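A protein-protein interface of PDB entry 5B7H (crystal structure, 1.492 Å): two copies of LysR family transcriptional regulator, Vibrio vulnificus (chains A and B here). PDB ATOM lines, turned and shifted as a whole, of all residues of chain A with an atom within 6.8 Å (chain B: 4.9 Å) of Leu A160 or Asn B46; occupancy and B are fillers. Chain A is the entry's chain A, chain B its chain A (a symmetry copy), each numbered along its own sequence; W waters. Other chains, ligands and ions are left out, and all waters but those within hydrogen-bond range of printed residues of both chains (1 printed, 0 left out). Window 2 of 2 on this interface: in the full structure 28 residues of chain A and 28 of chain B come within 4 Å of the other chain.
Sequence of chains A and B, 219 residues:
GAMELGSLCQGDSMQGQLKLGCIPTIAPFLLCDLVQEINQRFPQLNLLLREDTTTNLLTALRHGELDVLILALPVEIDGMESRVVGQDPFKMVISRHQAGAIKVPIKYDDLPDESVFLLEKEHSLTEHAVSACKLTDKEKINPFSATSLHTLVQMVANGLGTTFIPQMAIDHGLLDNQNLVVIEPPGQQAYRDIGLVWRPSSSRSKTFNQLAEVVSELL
The side-chain amide nitrogen (ND2) of Asn A158 sits close to the backbone NH (N) of Leu B47, at 2.9 Å.
The backbone NH (N) of Leu B18 sits at hydrogen-bond distance from the backbone carbonyl oxygen (O) of Asn B46 (2.9 Å). The backbone carbonyl oxygen (O) of Gly B16 is in hydrogen-bond range of the backbone NH (N) of Asn B46. The backbone NH (N) of Leu B48 is in hydrogen-bond range of the backbone carbonyl oxygen (O) of Leu B18 (2.9 Å). The backbone carbonyl oxygen (O) of Thr A162 is in hydrogen-bond range of the backbone NH (N) of Phe A117. The backbone carbonyl oxygen (O) of Met A155 is in hydrogen-bond range of the backbone NH (N) of Leu A160 (3.2 Å).
Among the printed residues, pairs that only touch across the chains: Phe A117 with Leu B48, Met A155 with Leu B47, Met A155 with Leu B48, Asn A158 with Leu B45, Asn A158 with Asn B46, Leu A160 with Asn B46 and Leu A160 with Leu B47.
Of the printed residues of chain B, Phe A117 touches Leu B48 (3.9 Å). Of the printed residues of chain B, Leu A160 touches Asn B46 (3.4 Å) and Leu B47 (3.5 Å). Of the printed residues of chain A, Leu B45 touches Asn A158. Asn B46 touches just these residues of chain A: Asn A158 (3.6 Å) and Leu A160 (3.4 Å). Of the printed residues of chain A, Leu B47 touches Met A155, Asn A158 and Leu A160.
Of the 8 printed residues of chain B, 4 touch a printed residue of chain A. Printed residues of chain B that touch a printed residue of chain A: Leu B45, Asn B46, Leu B47 and Leu B48. Hydrophobic or aromatic side chains of chain B within 4 Å of the printed part of chain A: Leu B47 and Leu B48. Among the printed residues, 8 pairs touch across the chains.
No position is printed for both chains.
Water W1 lies within hydrogen-bond range of O of Leu B45 (2.7 Å) and OD1 of Asn A158 (3.2 Å).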
ATOM      1  N   SER A  95      -4.563  -6.865 -21.147  1.00  0.00           N
ATOM      2  CA  SER A  95      -4.393  -5.470 -21.530  1.00  0.00           C
ATOM      3  C   SER A  95      -3.592  -5.348 -22.825  1.00  0.00           C
ATOM      4  O   SER A  95      -2.692  -6.145 -23.121  1.00  0.00           O
ATOM      5  CB  SER A  95      -3.715  -4.692 -20.414  1.00  0.00           C
ATOM      6  OG  SER A  95      -2.377  -5.111 -20.298  1.00  0.00           O
ATOM      7  N   GLN A  98       0.077  -5.405 -22.380  1.00  0.00           N
ATOM      8  CA  GLN A  98       0.617  -6.699 -21.976  1.00  0.00           C
ATOM      9  C   GLN A  98       0.525  -7.699 -23.107  1.00  0.00           C
ATOM     10  O   GLN A  98       0.913  -8.858 -22.923  1.00  0.00           O
ATOM     11  CB  GLN A  98      -0.181  -7.259 -20.774  1.00  0.00           C
ATOM     12  CG  GLN A  98       0.323  -6.774 -19.412  1.00  0.00           C
ATOM     13  CD  GLN A  98       1.602  -7.487 -19.041  1.00  0.00           C
ATOM     14  OE1 GLN A  98       1.874  -8.560 -19.576  1.00  0.00           O
ATOM     15  NE2 GLN A  98       2.407  -6.894 -18.151  1.00  0.00           N
ATOM     16  N   GLU A 114       0.827 -17.670 -11.528  1.00  0.00           N
ATOM     17  CA  GLU A 114      -0.011 -16.677 -10.835  1.00  0.00           C
ATOM     18  C   GLU A 114      -0.457 -15.548 -11.756  1.00  0.00           C
ATOM     19  O   GLU A 114      -0.739 -14.440 -11.291  1.00  0.00           O
ATOM     20  CB  GLU A 114       0.672 -16.053  -9.606  1.00  0.00           C
ATOM     21  CG  GLU A 114       1.308 -17.047  -8.673  1.00  0.00           C
ATOM     22  CD  GLU A 114       1.663 -16.473  -7.297  1.00  0.00           C
ATOM     23  OE1 GLU A 114       1.863 -17.283  -6.368  1.00  0.00           O
ATOM     24  OE2 GLU A 114       1.722 -15.237  -7.131  1.00  0.00           O
ATOM     25  N   SER A 115      -0.573 -15.788 -13.055  1.00  0.00           N
ATOM     26  CA  SER A 115      -1.030 -14.721 -13.953  1.00  0.00           C
ATOM     27  C   SER A 115      -2.514 -14.755 -14.259  1.00  0.00           C
ATOM     28  O   SER A 115      -3.019 -13.813 -14.876  1.00  0.00           O
ATOM     29  CB  SER A 115      -0.239 -14.743 -15.264  1.00  0.00           C
ATOM     30  OG  SER A 115      -0.430 -16.001 -15.939  1.00  0.00           O
ATOM     31  N   VAL A 116      -3.219 -15.813 -13.881  1.00  0.00           N
ATOM     32  CA  VAL A 116      -4.646 -15.945 -14.181  1.00  0.00           C
ATOM     33  C   VAL A 116      -5.428 -15.552 -12.942  1.00  0.00           C
ATOM     34  O   VAL A 116      -5.319 -16.217 -11.906  1.00  0.00           O
ATOM     35  CB  VAL A 116      -4.984 -17.380 -14.602  1.00  0.00           C
ATOM     36  CG1 VAL A 116      -6.499 -17.489 -14.831  1.00  0.00           C
ATOM     37  CG2 VAL A 116      -4.212 -17.720 -15.819  1.00  0.00           C
ATOM     38  N   PHE A 117      -6.222 -14.488 -13.027  1.00  0.00           N
ATOM     39  CA  PHE A 117      -7.030 -14.039 -11.896  1.00  0.00           C
ATOM     40  C   PHE A 117      -8.442 -14.603 -12.055  1.00  0.00           C
ATOM     41  O   PHE A 117      -8.964 -14.698 -13.177  1.00  0.00           O
ATOM     42  CB  PHE A 117      -7.089 -12.494 -11.848  1.00  0.00           C
ATOM     43  CG  PHE A 117      -5.823 -11.861 -11.340  1.00  0.00           C
ATOM     44  CD1 PHE A 117      -5.761 -11.423 -10.002  1.00  0.00           C
ATOM     45  CD2 PHE A 117      -4.662 -11.791 -12.143  1.00  0.00           C
ATOM     46  CE1 PHE A 117      -4.584 -10.809  -9.500  1.00  0.00           C
ATOM     47  CE2 PHE A 117      -3.477 -11.197 -11.660  1.00  0.00           C
ATOM     48  CZ  PHE A 117      -3.440 -10.719 -10.331  1.00  0.00           C
ATOM     49  N   ASN A 142      -3.533 -16.835  -9.854  1.00  0.00           N
ATOM     50  CA  ASN A 142      -3.067 -15.902  -8.842  1.00  0.00           C
ATOM     51  C   ASN A 142      -3.797 -16.146  -7.521  1.00  0.00           C
ATOM     52  O   ASN A 142      -5.014 -16.362  -7.505  1.00  0.00           O
ATOM     53  CB  ASN A 142      -3.344 -14.456  -9.289  1.00  0.00           C
ATOM     54  CG  ASN A 142      -2.591 -13.446  -8.409  1.00  0.00           C
ATOM     55  OD1 ASN A 142      -3.011 -13.175  -7.278  1.00  0.00           O
ATOM     56  ND2 ASN A 142      -1.442 -12.949  -8.901  1.00  0.00           N
ATOM     57  N   GLN A 154     -10.889  -4.862 -14.185  1.00  0.00           N
ATOM     58  CA  GLN A 154     -10.030  -3.711 -13.908  1.00  0.00           C
ATOM     59  C   GLN A 154      -8.614  -4.144 -13.534  1.00  0.00           C
ATOM     60  O   GLN A 154      -7.648  -3.488 -13.930  1.00  0.00           O
ATOM     61  CB  GLN A 154     -10.619  -2.840 -12.801  1.00  0.00           C
ATOM     62  CG  GLN A 154     -11.893  -2.098 -13.258  1.00  0.00           C
ATOM     63  CD  GLN A 154     -12.862  -1.783 -12.131  1.00  0.00           C
ATOM     64  OE1 GLN A 154     -12.646  -2.180 -10.967  1.00  0.00           O
ATOM     65  NE2 GLN A 154     -13.966  -1.155 -12.486  1.00  0.00           N
ATOM     66  N   MET A 155      -8.455  -5.226 -12.772  1.00  0.00           N
ATOM     67  CA  MET A 155      -7.095  -5.707 -12.487  1.00  0.00           C
ATOM     68  C   MET A 155      -6.383  -6.160 -13.758  1.00  0.00           C
ATOM     69  O   MET A 155      -5.184  -5.896 -13.934  1.00  0.00           O
ATOM     70  CB  MET A 155      -7.087  -6.838 -11.462  1.00  0.00           C
ATOM     71  CG  MET A 155      -7.449  -6.345 -10.070  1.00  0.00           C
ATOM     72  SD  MET A 155      -7.273  -7.585  -8.788  1.00  0.00           S
ATOM     73  CE  MET A 155      -8.693  -8.635  -9.100  1.00  0.00           C
ATOM     74  N   VAL A 156      -7.109  -6.814 -14.674  1.00  0.00           N
ATOM     75  CA  VAL A 156      -6.501  -7.174 -15.955  1.00  0.00           C
ATOM     76  C   VAL A 156      -6.137  -5.907 -16.711  1.00  0.00           C
ATOM     77  O   VAL A 156      -5.060  -5.816 -17.319  1.00  0.00           O
ATOM     78  CB  VAL A 156      -7.465  -8.089 -16.738  1.00  0.00           C
ATOM     79  CG1 VAL A 156      -6.942  -8.312 -18.184  1.00  0.00           C
ATOM     80  CG2 VAL A 156      -7.594  -9.450 -16.023  1.00  0.00           C
ATOM     81  N   ALA A 157      -7.043  -4.909 -16.704  1.00  0.00           N
ATOM     82  CA  ALA A 157      -6.744  -3.628 -17.367  1.00  0.00           C
ATOM     83  C   ALA A 157      -5.536  -2.918 -16.774  1.00  0.00           C
ATOM     84  O   ALA A 157      -4.867  -2.140 -17.457  1.00  0.00           O
ATOM     85  CB  ALA A 157      -7.959  -2.711 -17.384  1.00  0.00           C
ATOM     86  N   ASN A 158      -5.268  -3.130 -15.480  1.00  0.00           N
ATOM     87  CA  ASN A 158      -4.059  -2.579 -14.865  1.00  0.00           C
ATOM     88  C   ASN A 158      -2.791  -3.336 -15.268  1.00  0.00           C
ATOM     89  O   ASN A 158      -1.691  -2.968 -14.805  1.00  0.00           O
ATOM     90  CB  ASN A 158      -4.283  -2.671 -13.330  1.00  0.00           C
ATOM     91  CG  ASN A 158      -3.248  -1.884 -12.498  1.00  0.00           C
ATOM     92  OD1 ASN A 158      -2.848  -0.706 -12.785  1.00  0.00           O
ATOM     93  ND2 ASN A 158      -2.921  -2.477 -11.419  1.00  0.00           N
ATOM     94  N   GLY A 159      -2.925  -4.435 -16.015  1.00  0.00           N
ATOM     95  CA  GLY A 159      -1.786  -5.176 -16.531  1.00  0.00           C
ATOM     96  C   GLY A 159      -1.346  -6.341 -15.671  1.00  0.00           C
ATOM     97  O   GLY A 159      -0.242  -6.880 -15.888  1.00  0.00           O
ATOM     98  N   LEU A 160      -2.194  -6.790 -14.743  1.00  0.00           N
ATOM     99  CA  LEU A 160      -1.736  -7.765 -13.746  1.00  0.00           C
ATOM    100  C   LEU A 160      -1.759  -9.197 -14.273  1.00  0.00           C
ATOM    101  O   LEU A 160      -1.080 -10.074 -13.726  1.00  0.00           O
ATOM    102  CB  LEU A 160      -2.521  -7.616 -12.445  1.00  0.00           C
ATOM    103  CG  LEU A 160      -2.554  -6.197 -11.867  1.00  0.00           C
ATOM    104  CD1 LEU A 160      -3.228  -6.219 -10.473  1.00  0.00           C
ATOM    105  CD2 LEU A 160      -1.103  -5.617 -11.834  1.00  0.00           C
ATOM    106  N   GLY A 161      -2.486  -9.449 -15.358  1.00  0.00           N
ATOM    107  CA  GLY A 161      -2.534 -10.802 -15.876  1.00  0.00           C
ATOM    108  C   GLY A 161      -3.729 -10.960 -16.787  1.00  0.00           C
ATOM    109  O   GLY A 161      -4.057 -10.053 -17.563  1.00  0.00           O
ATOM    110  N   THR A 162      -4.367 -12.114 -16.750  1.00  0.00           N
ATOM    111  CA  THR A 162      -5.436 -12.412 -17.704  1.00  0.00           C
ATOM    112  C   THR A 162      -6.596 -13.050 -16.952  1.00  0.00           C
ATOM    113  O   THR A 162      -6.465 -13.442 -15.788  1.00  0.00           O
ATOM    114  CB  THR A 162      -4.911 -13.344 -18.812  1.00  0.00           C
ATOM    115  OG1 THR A 162      -5.923 -13.528 -19.810  1.00  0.00           O
ATOM    116  CG2 THR A 162      -4.490 -14.753 -18.279  1.00  0.00           C
ATOM    117  N   GLY B  16       4.937  -0.635  -6.447  1.00  0.00           N
ATOM    118  CA  GLY B  16       4.647  -1.837  -5.706  1.00  0.00           C
ATOM    119  C   GLY B  16       3.162  -2.137  -5.719  1.00  0.00           C
ATOM    120  O   GLY B  16       2.430  -1.709  -6.608  1.00  0.00           O
ATOM    121  N   GLN B  17       2.685  -2.814  -4.697  1.00  0.00           N
ATOM    122  CA  GLN B  17       1.329  -3.337  -4.706  1.00  0.00           C
ATOM    123  C   GLN B  17       0.491  -2.629  -3.651  1.00  0.00           C
ATOM    124  O   GLN B  17       0.977  -2.316  -2.563  1.00  0.00           O
ATOM    125  CB  GLN B  17       1.405  -4.804  -4.429  1.00  0.00           C
ATOM    126  CG  GLN B  17       0.128  -5.532  -4.403  1.00  0.00           C
ATOM    127  CD  GLN B  17       0.387  -6.986  -4.125  1.00  0.00           C
ATOM    128  OE1 GLN B  17       0.713  -7.752  -5.043  1.00  0.00           O
ATOM    129  NE2 GLN B  17       0.259  -7.383  -2.854  1.00  0.00           N
ATOM    130  N   LEU B  18      -0.773  -2.360  -3.991  1.00  0.00           N
ATOM    131  CA  LEU B  18      -1.729  -1.788  -3.060  1.00  0.00           C
ATOM    132  C   LEU B  18      -3.005  -2.615  -3.144  1.00  0.00           C
ATOM    133  O   LEU B  18      -3.445  -2.907  -4.259  1.00  0.00           O
ATOM    134  CB  LEU B  18      -1.998  -0.347  -3.486  1.00  0.00           C
ATOM    135  CG  LEU B  18      -2.554   0.654  -2.520  1.00  0.00           C
ATOM    136  CD1 LEU B  18      -1.558   0.768  -1.376  1.00  0.00           C
ATOM    137  CD2 LEU B  18      -2.695   1.975  -3.265  1.00  0.00           C
ATOM    138  N   GLN B  44       4.270   1.550 -12.188  1.00  0.00           N
ATOM    139  CA  GLN B  44       4.752   0.479 -11.319  1.00  0.00           C
ATOM    140  C   GLN B  44       3.835   0.210 -10.137  1.00  0.00           C
ATOM    141  O   GLN B  44       4.207  -0.556  -9.241  1.00  0.00           O
ATOM    142  CB  GLN B  44       6.171   0.746 -10.820  1.00  0.00           C
ATOM    143  CG  GLN B  44       7.233   0.271 -11.796  1.00  0.00           C
ATOM    144  CD  GLN B  44       7.293   1.170 -12.976  1.00  0.00           C
ATOM    145  OE1 GLN B  44       7.529   2.370 -12.825  1.00  0.00           O
ATOM    146  NE2 GLN B  44       7.044   0.623 -14.166  1.00  0.00           N
ATOM    147  N   LEU B  45       2.658   0.810 -10.111  1.00  0.00           N
ATOM    148  CA  LEU B  45       1.684   0.548  -9.064  1.00  0.00           C
ATOM    149  C   LEU B  45       0.719  -0.536  -9.516  1.00  0.00           C
ATOM    150  O   LEU B  45       0.041  -0.382 -10.544  1.00  0.00           O
ATOM    151  CB  LEU B  45       0.896   1.809  -8.725  1.00  0.00           C
ATOM    152  CG  LEU B  45      -0.036   1.702  -7.517  1.00  0.00           C
ATOM    153  CD1 LEU B  45       0.716   1.305  -6.236  1.00  0.00           C
ATOM    154  CD2 LEU B  45      -0.713   3.029  -7.343  1.00  0.00           C
ATOM    155  N   ASN B  46       0.664  -1.629  -8.757  1.00  0.00           N
ATOM    156  CA  ASN B  46      -0.221  -2.750  -9.062  1.00  0.00           C
ATOM    157  C   ASN B  46      -1.368  -2.672  -8.075  1.00  0.00           C
ATOM    158  O   ASN B  46      -1.137  -2.702  -6.860  1.00  0.00           O
ATOM    159  CB  ASN B  46       0.506  -4.088  -8.904  1.00  0.00           C
ATOM    160  CG  ASN B  46       1.465  -4.359 -10.042  1.00  0.00           C
ATOM    161  OD1 ASN B  46       1.592  -3.549 -10.956  1.00  0.00           O
ATOM    162  ND2 ASN B  46       2.125  -5.497 -10.007  1.00  0.00           N
ATOM    163  N   LEU B  47      -2.603  -2.562  -8.578  1.00  0.00           N
ATOM    164  CA  LEU B  47      -3.760  -2.348  -7.730  1.00  0.00           C
ATOM    165  C   LEU B  47      -4.566  -3.636  -7.661  1.00  0.00           C
ATOM    166  O   LEU B  47      -5.248  -3.988  -8.627  1.00  0.00           O
ATOM    167  CB  LEU B  47      -4.578  -1.184  -8.301  1.00  0.00           C
ATOM    168  CG  LEU B  47      -5.417  -0.266  -7.458  1.00  0.00           C
ATOM    169  CD1 LEU B  47      -4.613   0.313  -6.297  1.00  0.00           C
ATOM    170  CD2 LEU B  47      -5.939   0.820  -8.391  1.00  0.00           C
ATOM    171  N   LEU B  48      -4.500  -4.344  -6.527  1.00  0.00           N
ATOM    172  CA  LEU B  48      -5.328  -5.510  -6.246  1.00  0.00           C
ATOM    173  C   LEU B  48      -6.627  -4.959  -5.681  1.00  0.00           C
ATOM    174  O   LEU B  48      -6.594  -4.049  -4.843  1.00  0.00           O
ATOM    175  CB  LEU B  48      -4.647  -6.436  -5.224  1.00  0.00           C
ATOM    176  CG  LEU B  48      -3.355  -7.036  -5.779  1.00  0.00           C
ATOM    177  CD1 LEU B  48      -2.729  -7.857  -4.687  1.00  0.00           C
ATOM    178  CD2 LEU B  48      -3.702  -8.006  -6.911  1.00  0.00           C
HETATM  179  O   HOH W   1      -0.323   1.227 -12.631  1.00  0.00           O
